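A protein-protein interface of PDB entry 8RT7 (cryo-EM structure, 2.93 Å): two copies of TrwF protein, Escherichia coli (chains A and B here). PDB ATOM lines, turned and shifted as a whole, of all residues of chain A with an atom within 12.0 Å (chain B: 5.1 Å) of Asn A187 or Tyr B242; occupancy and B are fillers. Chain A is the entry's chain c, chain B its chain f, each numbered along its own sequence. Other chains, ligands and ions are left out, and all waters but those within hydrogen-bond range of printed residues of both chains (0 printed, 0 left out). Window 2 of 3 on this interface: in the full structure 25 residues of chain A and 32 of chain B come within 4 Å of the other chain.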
ATOM      1  N   LYS A 166       5.042 -27.875  -2.706  1.00  0.00           N
ATOM      2  CA  LYS A 166       4.224 -28.348  -3.815  1.00  0.00           C
ATOM      3  C   LYS A 166       2.822 -27.769  -3.824  1.00  0.00           C
ATOM      4  O   LYS A 166       2.071 -28.041  -4.763  1.00  0.00           O
ATOM      5  CB  LYS A 166       4.120 -29.867  -3.788  1.00  0.00           C
ATOM      6  CG  LYS A 166       5.440 -30.568  -3.686  1.00  0.00           C
ATOM      7  CD  LYS A 166       6.249 -30.391  -4.935  1.00  0.00           C
ATOM      8  CE  LYS A 166       7.556 -31.114  -4.796  1.00  0.00           C
ATOM      9  NZ  LYS A 166       7.311 -32.548  -4.528  1.00  0.00           N
ATOM     10  N   ASP A 167       2.437 -27.004  -2.807  1.00  0.00           N
ATOM     11  CA  ASP A 167       1.105 -26.421  -2.824  1.00  0.00           C
ATOM     12  C   ASP A 167       0.996 -25.271  -3.811  1.00  0.00           C
ATOM     13  O   ASP A 167      -0.116 -24.926  -4.214  1.00  0.00           O
ATOM     14  CB  ASP A 167       0.704 -25.978  -1.418  1.00  0.00           C
ATOM     15  CG  ASP A 167       1.724 -25.075  -0.772  1.00  0.00           C
ATOM     16  OD1 ASP A 167       2.422 -25.531   0.154  1.00  0.00           O
ATOM     17  OD2 ASP A 167       1.813 -23.900  -1.167  1.00  0.00           O
ATOM     18  N   ILE A 168       2.118 -24.693  -4.235  1.00  0.00           N
ATOM     19  CA  ILE A 168       2.127 -23.662  -5.262  1.00  0.00           C
ATOM     20  C   ILE A 168       2.620 -24.199  -6.597  1.00  0.00           C
ATOM     21  O   ILE A 168       2.897 -23.419  -7.507  1.00  0.00           O
ATOM     22  CB  ILE A 168       2.960 -22.446  -4.830  1.00  0.00           C
ATOM     23  CG1 ILE A 168       4.397 -22.852  -4.545  1.00  0.00           C
ATOM     24  CG2 ILE A 168       2.355 -21.786  -3.617  1.00  0.00           C
ATOM     25  CD1 ILE A 168       5.313 -21.694  -4.482  1.00  0.00           C
ATOM     26  N   ALA A 169       2.728 -25.512  -6.740  1.00  0.00           N
ATOM     27  CA  ALA A 169       3.311 -26.095  -7.931  1.00  0.00           C
ATOM     28  C   ALA A 169       2.404 -25.909  -9.144  1.00  0.00           C
ATOM     29  O   ALA A 169       1.184 -25.809  -9.008  1.00  0.00           O
ATOM     30  CB  ALA A 169       3.566 -27.577  -7.715  1.00  0.00           C
ATOM     31  N   PRO A 170       2.976 -25.855 -10.344  1.00  0.00           N
ATOM     32  CA  PRO A 170       2.160 -25.892 -11.557  1.00  0.00           C
ATOM     33  C   PRO A 170       1.711 -27.310 -11.859  1.00  0.00           C
ATOM     34  O   PRO A 170       2.272 -28.287 -11.367  1.00  0.00           O
ATOM     35  CB  PRO A 170       3.115 -25.386 -12.642  1.00  0.00           C
ATOM     36  CG  PRO A 170       4.280 -24.848 -11.929  1.00  0.00           C
ATOM     37  CD  PRO A 170       4.386 -25.613 -10.671  1.00  0.00           C
ATOM     38  N   VAL A 171       0.681 -27.414 -12.692  1.00  0.00           N
ATOM     39  CA  VAL A 171       0.257 -28.726 -13.153  1.00  0.00           C
ATOM     40  C   VAL A 171       1.055 -29.187 -14.362  1.00  0.00           C
ATOM     41  O   VAL A 171       1.117 -30.394 -14.622  1.00  0.00           O
ATOM     42  CB  VAL A 171      -1.245 -28.756 -13.487  1.00  0.00           C
ATOM     43  CG1 VAL A 171      -2.050 -28.403 -12.275  1.00  0.00           C
ATOM     44  CG2 VAL A 171      -1.560 -27.814 -14.609  1.00  0.00           C
ATOM     45  N   LYS A 183       1.816 -23.993 -16.433  1.00  0.00           N
ATOM     46  CA  LYS A 183       0.364 -24.031 -16.384  1.00  0.00           C
ATOM     47  C   LYS A 183      -0.080 -24.267 -14.950  1.00  0.00           C
ATOM     48  O   LYS A 183       0.393 -25.199 -14.297  1.00  0.00           O
ATOM     49  CB  LYS A 183      -0.183 -25.123 -17.294  1.00  0.00           C
ATOM     50  CG  LYS A 183      -1.649 -24.993 -17.579  1.00  0.00           C
ATOM     51  CD  LYS A 183      -2.044 -25.798 -18.784  1.00  0.00           C
ATOM     52  CE  LYS A 183      -2.321 -27.220 -18.407  1.00  0.00           C
ATOM     53  NZ  LYS A 183      -3.578 -27.314 -17.642  1.00  0.00           N
ATOM     54  N   PHE A 184      -0.974 -23.420 -14.462  1.00  0.00           N
ATOM     55  CA  PHE A 184      -1.496 -23.535 -13.113  1.00  0.00           C
ATOM     56  C   PHE A 184      -2.980 -23.861 -13.167  1.00  0.00           C
ATOM     57  O   PHE A 184      -3.693 -23.433 -14.075  1.00  0.00           O
ATOM     58  CB  PHE A 184      -1.254 -22.247 -12.326  1.00  0.00           C
ATOM     59  CG  PHE A 184       0.195 -21.952 -12.091  1.00  0.00           C
ATOM     60  CD1 PHE A 184       0.931 -21.254 -13.019  1.00  0.00           C
ATOM     61  CD2 PHE A 184       0.821 -22.373 -10.942  1.00  0.00           C
ATOM     62  CE1 PHE A 184       2.254 -20.992 -12.811  1.00  0.00           C
ATOM     63  CE2 PHE A 184       2.142 -22.108 -10.735  1.00  0.00           C
ATOM     64  CZ  PHE A 184       2.857 -21.419 -11.670  1.00  0.00           C
ATOM     65  N   SER A 185      -3.440 -24.645 -12.198  1.00  0.00           N
ATOM     66  CA  SER A 185      -4.830 -25.064 -12.177  1.00  0.00           C
ATOM     67  C   SER A 185      -5.740 -23.868 -11.906  1.00  0.00           C
ATOM     68  O   SER A 185      -5.288 -22.741 -11.702  1.00  0.00           O
ATOM     69  CB  SER A 185      -5.029 -26.162 -11.142  1.00  0.00           C
ATOM     70  OG  SER A 185      -4.603 -25.729  -9.869  1.00  0.00           O
ATOM     71  N   ALA A 186      -7.049 -24.114 -11.920  1.00  0.00           N
ATOM     72  CA  ALA A 186      -8.005 -23.017 -11.817  1.00  0.00           C
ATOM     73  C   ALA A 186      -8.092 -22.475 -10.398  1.00  0.00           C
ATOM     74  O   ALA A 186      -8.270 -21.270 -10.198  1.00  0.00           O
ATOM     75  CB  ALA A 186      -9.376 -23.470 -12.297  1.00  0.00           C
ATOM     76  N   ASN A 187      -7.967 -23.343  -9.403  1.00  0.00           N
ATOM     77  CA  ASN A 187      -8.108 -22.959  -8.007  1.00  0.00           C
ATOM     78  C   ASN A 187      -6.809 -22.466  -7.399  1.00  0.00           C
ATOM     79  O   ASN A 187      -6.758 -22.235  -6.190  1.00  0.00           O
ATOM     80  CB  ASN A 187      -8.635 -24.135  -7.188  1.00  0.00           C
ATOM     81  CG  ASN A 187     -10.078 -24.451  -7.484  1.00  0.00           C
ATOM     82  OD1 ASN A 187     -10.832 -23.597  -7.936  1.00  0.00           O
ATOM     83  ND2 ASN A 187     -10.468 -25.691  -7.242  1.00  0.00           N
ATOM     84  N   ALA A 188      -5.763 -22.308  -8.197  1.00  0.00           N
ATOM     85  CA  ALA A 188      -4.451 -21.938  -7.696  1.00  0.00           C
ATOM     86  C   ALA A 188      -4.188 -20.456  -7.904  1.00  0.00           C
ATOM     87  O   ALA A 188      -4.489 -19.904  -8.964  1.00  0.00           O
ATOM     88  CB  ALA A 188      -3.363 -22.749  -8.390  1.00  0.00           C
ATOM     89  N   ASP A 189      -3.639 -19.814  -6.877  1.00  0.00           N
ATOM     90  CA  ASP A 189      -3.082 -18.481  -7.034  1.00  0.00           C
ATOM     91  C   ASP A 189      -1.886 -18.536  -7.968  1.00  0.00           C
ATOM     92  O   ASP A 189      -1.086 -19.470  -7.917  1.00  0.00           O
ATOM     93  CB  ASP A 189      -2.646 -17.919  -5.687  1.00  0.00           C
ATOM     94  CG  ASP A 189      -3.808 -17.560  -4.797  1.00  0.00           C
ATOM     95  OD1 ASP A 189      -4.961 -17.696  -5.236  1.00  0.00           O
ATOM     96  OD2 ASP A 189      -3.569 -17.134  -3.651  1.00  0.00           O
ATOM     97  N   LEU A 190      -1.762 -17.538  -8.831  1.00  0.00           N
ATOM     98  CA  LEU A 190      -0.602 -17.475  -9.704  1.00  0.00           C
ATOM     99  C   LEU A 190       0.575 -16.885  -8.946  1.00  0.00           C
ATOM    100  O   LEU A 190       0.482 -15.755  -8.460  1.00  0.00           O
ATOM    101  CB  LEU A 190      -0.876 -16.651 -10.946  1.00  0.00           C
ATOM    102  CG  LEU A 190      -1.885 -17.197 -11.941  1.00  0.00           C
ATOM    103  CD1 LEU A 190      -2.044 -16.205 -13.053  1.00  0.00           C
ATOM    104  CD2 LEU A 190      -1.436 -18.532 -12.468  1.00  0.00           C
ATOM    105  N   PRO A 191       1.678 -17.592  -8.833  1.00  0.00           N
ATOM    106  CA  PRO A 191       2.810 -17.095  -8.053  1.00  0.00           C
ATOM    107  C   PRO A 191       3.714 -16.173  -8.843  1.00  0.00           C
ATOM    108  O   PRO A 191       3.405 -15.790  -9.971  1.00  0.00           O
ATOM    109  CB  PRO A 191       3.535 -18.380  -7.669  1.00  0.00           C
ATOM    110  CG  PRO A 191       3.268 -19.271  -8.800  1.00  0.00           C
ATOM    111  CD  PRO A 191       1.938 -18.930  -9.368  1.00  0.00           C
ATOM    112  N   SER A 213      -8.071 -19.154 -20.148  1.00  0.00           N
ATOM    113  CA  SER A 213      -8.486 -18.772 -18.811  1.00  0.00           C
ATOM    114  C   SER A 213      -7.367 -18.118 -18.020  1.00  0.00           C
ATOM    115  O   SER A 213      -7.439 -18.067 -16.790  1.00  0.00           O
ATOM    116  CB  SER A 213      -9.010 -19.991 -18.065  1.00  0.00           C
ATOM    117  OG  SER A 213      -7.984 -20.934 -17.886  1.00  0.00           O
ATOM    118  N   ASN A 214      -6.336 -17.627 -18.701  1.00  0.00           N
ATOM    119  CA  ASN A 214      -5.178 -17.005 -18.063  1.00  0.00           C
ATOM    120  C   ASN A 214      -4.520 -17.940 -17.060  1.00  0.00           C
ATOM    121  O   ASN A 214      -4.098 -17.522 -15.985  1.00  0.00           O
ATOM    122  CB  ASN A 214      -5.549 -15.686 -17.394  1.00  0.00           C
ATOM    123  CG  ASN A 214      -6.210 -14.728 -18.335  1.00  0.00           C
ATOM    124  OD1 ASN A 214      -7.405 -14.489 -18.248  1.00  0.00           O
ATOM    125  ND2 ASN A 214      -5.442 -14.183 -19.255  1.00  0.00           N
ATOM    126  N   ASN A 215      -4.427 -19.216 -17.410  1.00  0.00           N
ATOM    127  CA  ASN A 215      -3.864 -20.207 -16.510  1.00  0.00           C
ATOM    128  C   ASN A 215      -2.385 -20.462 -16.741  1.00  0.00           C
ATOM    129  O   ASN A 215      -1.790 -21.236 -15.993  1.00  0.00           O
ATOM    130  CB  ASN A 215      -4.629 -21.525 -16.630  1.00  0.00           C
ATOM    131  CG  ASN A 215      -4.830 -21.956 -18.057  1.00  0.00           C
ATOM    132  OD1 ASN A 215      -4.527 -21.221 -18.984  1.00  0.00           O
ATOM    133  ND2 ASN A 215      -5.335 -23.160 -18.241  1.00  0.00           N
ATOM    134  N   ILE A 216      -1.773 -19.832 -17.740  1.00  0.00           N
ATOM    135  CA  ILE A 216      -0.395 -20.113 -18.130  1.00  0.00           C
ATOM    136  C   ILE A 216       0.416 -18.834 -18.046  1.00  0.00           C
ATOM    137  O   ILE A 216       0.058 -17.827 -18.661  1.00  0.00           O
ATOM    138  CB  ILE A 216      -0.313 -20.697 -19.549  1.00  0.00           C
ATOM    139  CG1 ILE A 216      -1.044 -22.026 -19.631  1.00  0.00           C
ATOM    140  CG2 ILE A 216       1.110 -20.877 -19.948  1.00  0.00           C
ATOM    141  CD1 ILE A 216      -1.353 -22.435 -21.023  1.00  0.00           C
ATOM    142  N   LEU A 230       5.507 -17.762  -3.656  1.00  0.00           N
ATOM    143  CA  LEU A 230       4.186 -17.226  -3.338  1.00  0.00           C
ATOM    144  C   LEU A 230       4.108 -17.050  -1.828  1.00  0.00           C
ATOM    145  O   LEU A 230       3.924 -18.023  -1.095  1.00  0.00           O
ATOM    146  CB  LEU A 230       3.077 -18.134  -3.845  1.00  0.00           C
ATOM    147  CG  LEU A 230       1.657 -17.593  -3.715  1.00  0.00           C
ATOM    148  CD1 LEU A 230       1.593 -16.145  -4.106  1.00  0.00           C
ATOM    149  CD2 LEU A 230       0.730 -18.389  -4.568  1.00  0.00           C
ATOM    150  N   ARG A 233       6.435 -19.323   0.538  1.00  0.00           N
ATOM    151  CA  ARG A 233       6.567 -20.667   0.001  1.00  0.00           C
ATOM    152  C   ARG A 233       7.357 -20.611  -1.292  1.00  0.00           C
ATOM    153  O   ARG A 233       7.132 -19.732  -2.125  1.00  0.00           O
ATOM    154  CB  ARG A 233       5.205 -21.298  -0.237  1.00  0.00           C
ATOM    155  CG  ARG A 233       4.214 -20.944   0.836  1.00  0.00           C
ATOM    156  CD  ARG A 233       3.113 -21.962   0.960  1.00  0.00           C
ATOM    157  NE  ARG A 233       3.589 -23.336   1.074  1.00  0.00           N
ATOM    158  CZ  ARG A 233       4.182 -23.840   2.148  1.00  0.00           C
ATOM    159  NH1 ARG A 233       4.561 -25.105   2.158  1.00  0.00           N
ATOM    160  NH2 ARG A 233       4.405 -23.079   3.205  1.00  0.00           N
ATOM    161  N   GLY B 177     -17.607 -25.099  -7.131  1.00  0.00           N
ATOM    162  CA  GLY B 177     -16.444 -25.196  -7.971  1.00  0.00           C
ATOM    163  C   GLY B 177     -15.721 -23.887  -8.179  1.00  0.00           C
ATOM    164  O   GLY B 177     -14.527 -23.898  -8.476  1.00  0.00           O
ATOM    165  N   LYS B 221     -13.496 -17.608  -3.962  1.00  0.00           N
ATOM    166  CA  LYS B 221     -12.363 -18.508  -4.029  1.00  0.00           C
ATOM    167  C   LYS B 221     -12.762 -19.834  -3.405  1.00  0.00           C
ATOM    168  O   LYS B 221     -13.604 -19.882  -2.512  1.00  0.00           O
ATOM    169  CB  LYS B 221     -11.156 -17.897  -3.308  1.00  0.00           C
ATOM    170  CG  LYS B 221      -9.863 -18.654  -3.465  1.00  0.00           C
ATOM    171  CD  LYS B 221      -9.373 -18.583  -4.890  1.00  0.00           C
ATOM    172  CE  LYS B 221      -8.200 -19.501  -5.122  1.00  0.00           C
ATOM    173  NZ  LYS B 221      -7.138 -19.234  -4.140  1.00  0.00           N
ATOM    174  N   VAL B 222     -12.161 -20.913  -3.894  1.00  0.00           N
ATOM    175  CA  VAL B 222     -12.272 -22.231  -3.283  1.00  0.00           C
ATOM    176  C   VAL B 222     -10.936 -22.543  -2.630  1.00  0.00           C
ATOM    177  O   VAL B 222      -9.886 -22.428  -3.268  1.00  0.00           O
ATOM    178  CB  VAL B 222     -12.660 -23.309  -4.308  1.00  0.00           C
ATOM    179  CG1 VAL B 222     -12.362 -24.676  -3.765  1.00  0.00           C
ATOM    180  CG2 VAL B 222     -14.112 -23.212  -4.644  1.00  0.00           C
ATOM    181  N   ASN B 223     -10.975 -22.921  -1.357  1.00  0.00           N
ATOM    182  CA  ASN B 223      -9.784 -23.029  -0.532  1.00  0.00           C
ATOM    183  C   ASN B 223      -9.978 -24.177   0.442  1.00  0.00           C
ATOM    184  O   ASN B 223     -11.118 -24.503   0.783  1.00  0.00           O
ATOM    185  CB  ASN B 223      -9.542 -21.715   0.219  1.00  0.00           C
ATOM    186  CG  ASN B 223      -8.201 -21.654   0.871  1.00  0.00           C
ATOM    187  OD1 ASN B 223      -7.178 -21.758   0.212  1.00  0.00           O
ATOM    188  ND2 ASN B 223      -8.192 -21.476   2.179  1.00  0.00           N
ATOM    189  N   PRO B 224      -8.900 -24.822   0.892  1.00  0.00           N
ATOM    190  CA  PRO B 224      -9.070 -25.894   1.879  1.00  0.00           C
ATOM    191  C   PRO B 224      -9.476 -25.417   3.264  1.00  0.00           C
ATOM    192  O   PRO B 224     -10.189 -26.147   3.959  1.00  0.00           O
ATOM    193  CB  PRO B 224      -7.696 -26.574   1.902  1.00  0.00           C
ATOM    194  CG  PRO B 224      -6.781 -25.654   1.219  1.00  0.00           C
ATOM    195  CD  PRO B 224      -7.588 -24.903   0.238  1.00  0.00           C
ATOM    196  N   ASN B 239     -12.460 -27.452   4.208  1.00  0.00           N
ATOM    197  CA  ASN B 239     -12.954 -28.106   3.004  1.00  0.00           C
ATOM    198  C   ASN B 239     -12.314 -29.481   2.917  1.00  0.00           C
ATOM    199  O   ASN B 239     -11.122 -29.598   2.623  1.00  0.00           O
ATOM    200  CB  ASN B 239     -12.623 -27.268   1.777  1.00  0.00           C
ATOM    201  CG  ASN B 239     -13.271 -27.784   0.530  1.00  0.00           C
ATOM    202  OD1 ASN B 239     -13.991 -28.772   0.560  1.00  0.00           O
ATOM    203  ND2 ASN B 239     -13.028 -27.112  -0.580  1.00  0.00           N
ATOM    204  N   GLU B 240     -13.094 -30.524   3.182  1.00  0.00           N
ATOM    205  CA  GLU B 240     -12.555 -31.875   3.233  1.00  0.00           C
ATOM    206  C   GLU B 240     -12.447 -32.533   1.868  1.00  0.00           C
ATOM    207  O   GLU B 240     -11.933 -33.650   1.779  1.00  0.00           O
ATOM    208  CB  GLU B 240     -13.423 -32.744   4.134  1.00  0.00           C
ATOM    209  CG  GLU B 240     -13.632 -32.163   5.501  1.00  0.00           C
ATOM    210  CD  GLU B 240     -12.551 -32.556   6.475  1.00  0.00           C
ATOM    211  OE1 GLU B 240     -11.859 -31.660   6.993  1.00  0.00           O
ATOM    212  OE2 GLU B 240     -12.397 -33.766   6.733  1.00  0.00           O
ATOM    213  N   ALA B 241     -12.921 -31.884   0.815  1.00  0.00           N
ATOM    214  CA  ALA B 241     -12.901 -32.431  -0.532  1.00  0.00           C
ATOM    215  C   ALA B 241     -12.326 -31.415  -1.494  1.00  0.00           C
ATOM    216  O   ALA B 241     -12.881 -31.139  -2.557  1.00  0.00           O
ATOM    217  CB  ALA B 241     -14.295 -32.854  -0.968  1.00  0.00           C
ATOM    218  N   TYR B 242     -11.198 -30.827  -1.117  1.00  0.00           N
ATOM    219  CA  TYR B 242     -10.616 -29.763  -1.918  1.00  0.00           C
ATOM    220  C   TYR B 242     -10.124 -30.308  -3.249  1.00  0.00           C
ATOM    221  O   TYR B 242      -9.386 -31.296  -3.298  1.00  0.00           O
ATOM    222  CB  TYR B 242      -9.473 -29.097  -1.159  1.00  0.00           C
ATOM    223  CG  TYR B 242      -8.801 -28.008  -1.946  1.00  0.00           C
ATOM    224  CD1 TYR B 242      -9.524 -26.954  -2.464  1.00  0.00           C
ATOM    225  CD2 TYR B 242      -7.443 -28.039  -2.177  1.00  0.00           C
ATOM    226  CE1 TYR B 242      -8.914 -25.965  -3.190  1.00  0.00           C
ATOM    227  CE2 TYR B 242      -6.826 -27.052  -2.898  1.00  0.00           C
ATOM    228  CZ  TYR B 242      -7.566 -26.018  -3.401  1.00  0.00           C
ATOM    229  OH  TYR B 242      -6.944 -25.033  -4.119  1.00  0.00           O
ATOM    230  N   ASP B 243     -10.539 -29.658  -4.329  1.00  0.00           N
ATOM    231  CA  ASP B 243     -10.148 -30.044  -5.677  1.00  0.00           C
ATOM    232  C   ASP B 243      -9.207 -28.992  -6.232  1.00  0.00           C
ATOM    233  O   ASP B 243      -9.662 -27.897  -6.596  1.00  0.00           O
ATOM    234  CB  ASP B 243     -11.373 -30.183  -6.575  1.00  0.00           C
ATOM    235  CG  ASP B 243     -11.032 -30.714  -7.943  1.00  0.00           C
ATOM    236  OD1 ASP B 243      -9.972 -31.353  -8.085  1.00  0.00           O
ATOM    237  OD2 ASP B 243     -11.823 -30.495  -8.879  1.00  0.00           O
ATOM    238  N   PRO B 244      -7.903 -29.257  -6.304  1.00  0.00           N
ATOM    239  CA  PRO B 244      -6.976 -28.227  -6.791  1.00  0.00           C
ATOM    240  C   PRO B 244      -7.258 -27.790  -8.211  1.00  0.00           C
ATOM    241  O   PRO B 244      -7.023 -26.627  -8.551  1.00  0.00           O
ATOM    242  CB  PRO B 244      -5.609 -28.910  -6.676  1.00  0.00           C
ATOM    243  CG  PRO B 244      -5.814 -30.050  -5.752  1.00  0.00           C
ATOM    244  CD  PRO B 244      -7.206 -30.509  -5.983  1.00  0.00           C
ATOM    245  N   ASN B 245      -7.755 -28.691  -9.054  1.00  0.00           N
ATOM    246  CA  ASN B 245      -7.902 -28.379 -10.468  1.00  0.00           C
ATOM    247  C   ASN B 245      -9.048 -27.408 -10.713  1.00  0.00           C
ATOM    248  O   ASN B 245      -8.909 -26.458 -11.489  1.00  0.00           O
ATOM    249  CB  ASN B 245      -8.100 -29.669 -11.255  1.00  0.00           C
ATOM    250  CG  ASN B 245      -7.076 -30.713 -10.902  1.00  0.00           C
ATOM    251  OD1 ASN B 245      -5.875 -30.446 -10.915  1.00  0.00           O
ATOM    252  ND2 ASN B 245      -7.541 -31.908 -10.567  1.00  0.00           N
ATOM    253  N   GLY B 246     -10.184 -27.632 -10.081  1.00  0.00           N
ATOM    254  CA  GLY B 246     -11.295 -26.726 -10.263  1.00  0.00           C
ATOM    255  C   GLY B 246     -11.848 -26.776 -11.676  1.00  0.00           C
ATOM    256  O   GLY B 246     -11.552 -27.667 -12.466  1.00  0.00           O
ATOM    257  N   VAL B 247     -12.664 -25.776 -11.986  1.00  0.00           N
ATOM    258  CA  VAL B 247     -13.280 -25.632 -13.297  1.00  0.00           C
ATOM    259  C   VAL B 247     -12.731 -24.375 -13.963  1.00  0.00           C
ATOM    260  O   VAL B 247     -12.877 -23.274 -13.425  1.00  0.00           O
ATOM    261  CB  VAL B 247     -14.817 -25.597 -13.215  1.00  0.00           C
ATOM    262  CG1 VAL B 247     -15.337 -26.946 -12.783  1.00  0.00           C
ATOM    263  CG2 VAL B 247     -15.291 -24.549 -12.228  1.00  0.00           C
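Asp A167 touches none of the printed residues of chain B.
Of the printed residues of chain B, Ser A185 touches Pro B244 (2.9 Å) and Asn B245 (3.7 Å).
Printed residues of chain B within 4 Å of Ala A186: Asn B245 (3.0 Å) and Val B247 (3.7 Å).
Of chain B, only Gly B177 (3.7 Å), Lys B221 (3.3 Å), Tyr B242 (3.5 Å), Asp B243 (2.4 Å), Pro B244 (3.3 Å), Asn B245 (3.9 Å) and Gly B246 (3.3 Å) come within 4 Å of Asn A187.
Printed residues of chain B within 4 Å of Asp A189: Lys B221.
Ser A213 touches none of the printed residues of chain B.
Of chain A, only Asn A187 comes within 4 Å of Gly B177.
Lys B221 touches just these residues of chain A: Asn A187 and Asp A189.
No residue of chain A comes within 4 Å of Pro B224.
Ala B241 touches none of the printed residues of chain A.
Tyr B242 touches just one residue of chain A: Asn A187 (3.5 Å).
Asp B243 touches one residue of chain A.
Of the printed residues of chain A, Pro B244 touches Ser A185 and Asn A187.
Asn B245 touches three residues of chain A.
Gly B246 touches just one residue of chain A: Asn A187 (3.3 Å).
Val B247 touches just one residue of chain A: Ala A186 (3.7 Å).
The nearest residue of chain B that does not touch Asn A187 is Val B222 (4.1 Å).
The nearest residue of chain A that does not touch Tyr B242 is Ala A188 (5.0 Å).
Of the 21 printed residues of chain A, 4 touch a printed residue of chain B.
Printed residues of chain A that touch a printed residue of chain B: Ser A185, Ala A186, Asn A187 and Asp A189.
Hydrophobic or aromatic side chains of chain A within 4 Å of the printed part of chain B: Ala A186.
Hydrophobic or aromatic side chains of chain B that line the printed part of chain A: Tyr B242.
Among the printed residues, 12 pairs touch across the chains.
Among the printed residues, Asp or Glu carboxylates within 4 Å of a Lys or Arg side-chain nitrogen of the other chain: Asp A189 with Lys B221 (2.9 Å).
No position is printed for both chains.
O of Pro B244 is in hydrogen-bond range of OG of Ser A185, 2.9 Å away.
The backbone carbonyl oxygen (O) of Asn B245 sits at hydrogen-bond distance from the backbone NH (N) of Ala A186.
The side-chain hydroxyl of Tyr B242 lies within hydrogen-bond range of the backbone carbonyl oxygen of Asn A187, 3.5 Å away.
The backbone carbonyl oxygen (O) of Asp B243 is in hydrogen-bond range of the side-chain amide nitrogen (ND2) of Asn A187 (2.4 Å).
ND2 of Asn A187 lies close to N of Gly B246 (3.5 Å).
The side-chain carboxylate (OD1) of Asp A189 lies within salt-bridge range of the side-chain amino group (NZ) of Lys B221.
Among the printed residues, pairs that only touch across the chains: Asn A187 with Pro B244 (3.3 Å), Asn A187 with Lys B221 (3.3 Å), Ala A186 with Val B247 (3.7 Å), Ser A185 with Asn B245 (3.7 Å), Asn A187 with Gly B177 (3.7 Å) and Asn A187 with Asn B245 (3.9 Å).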
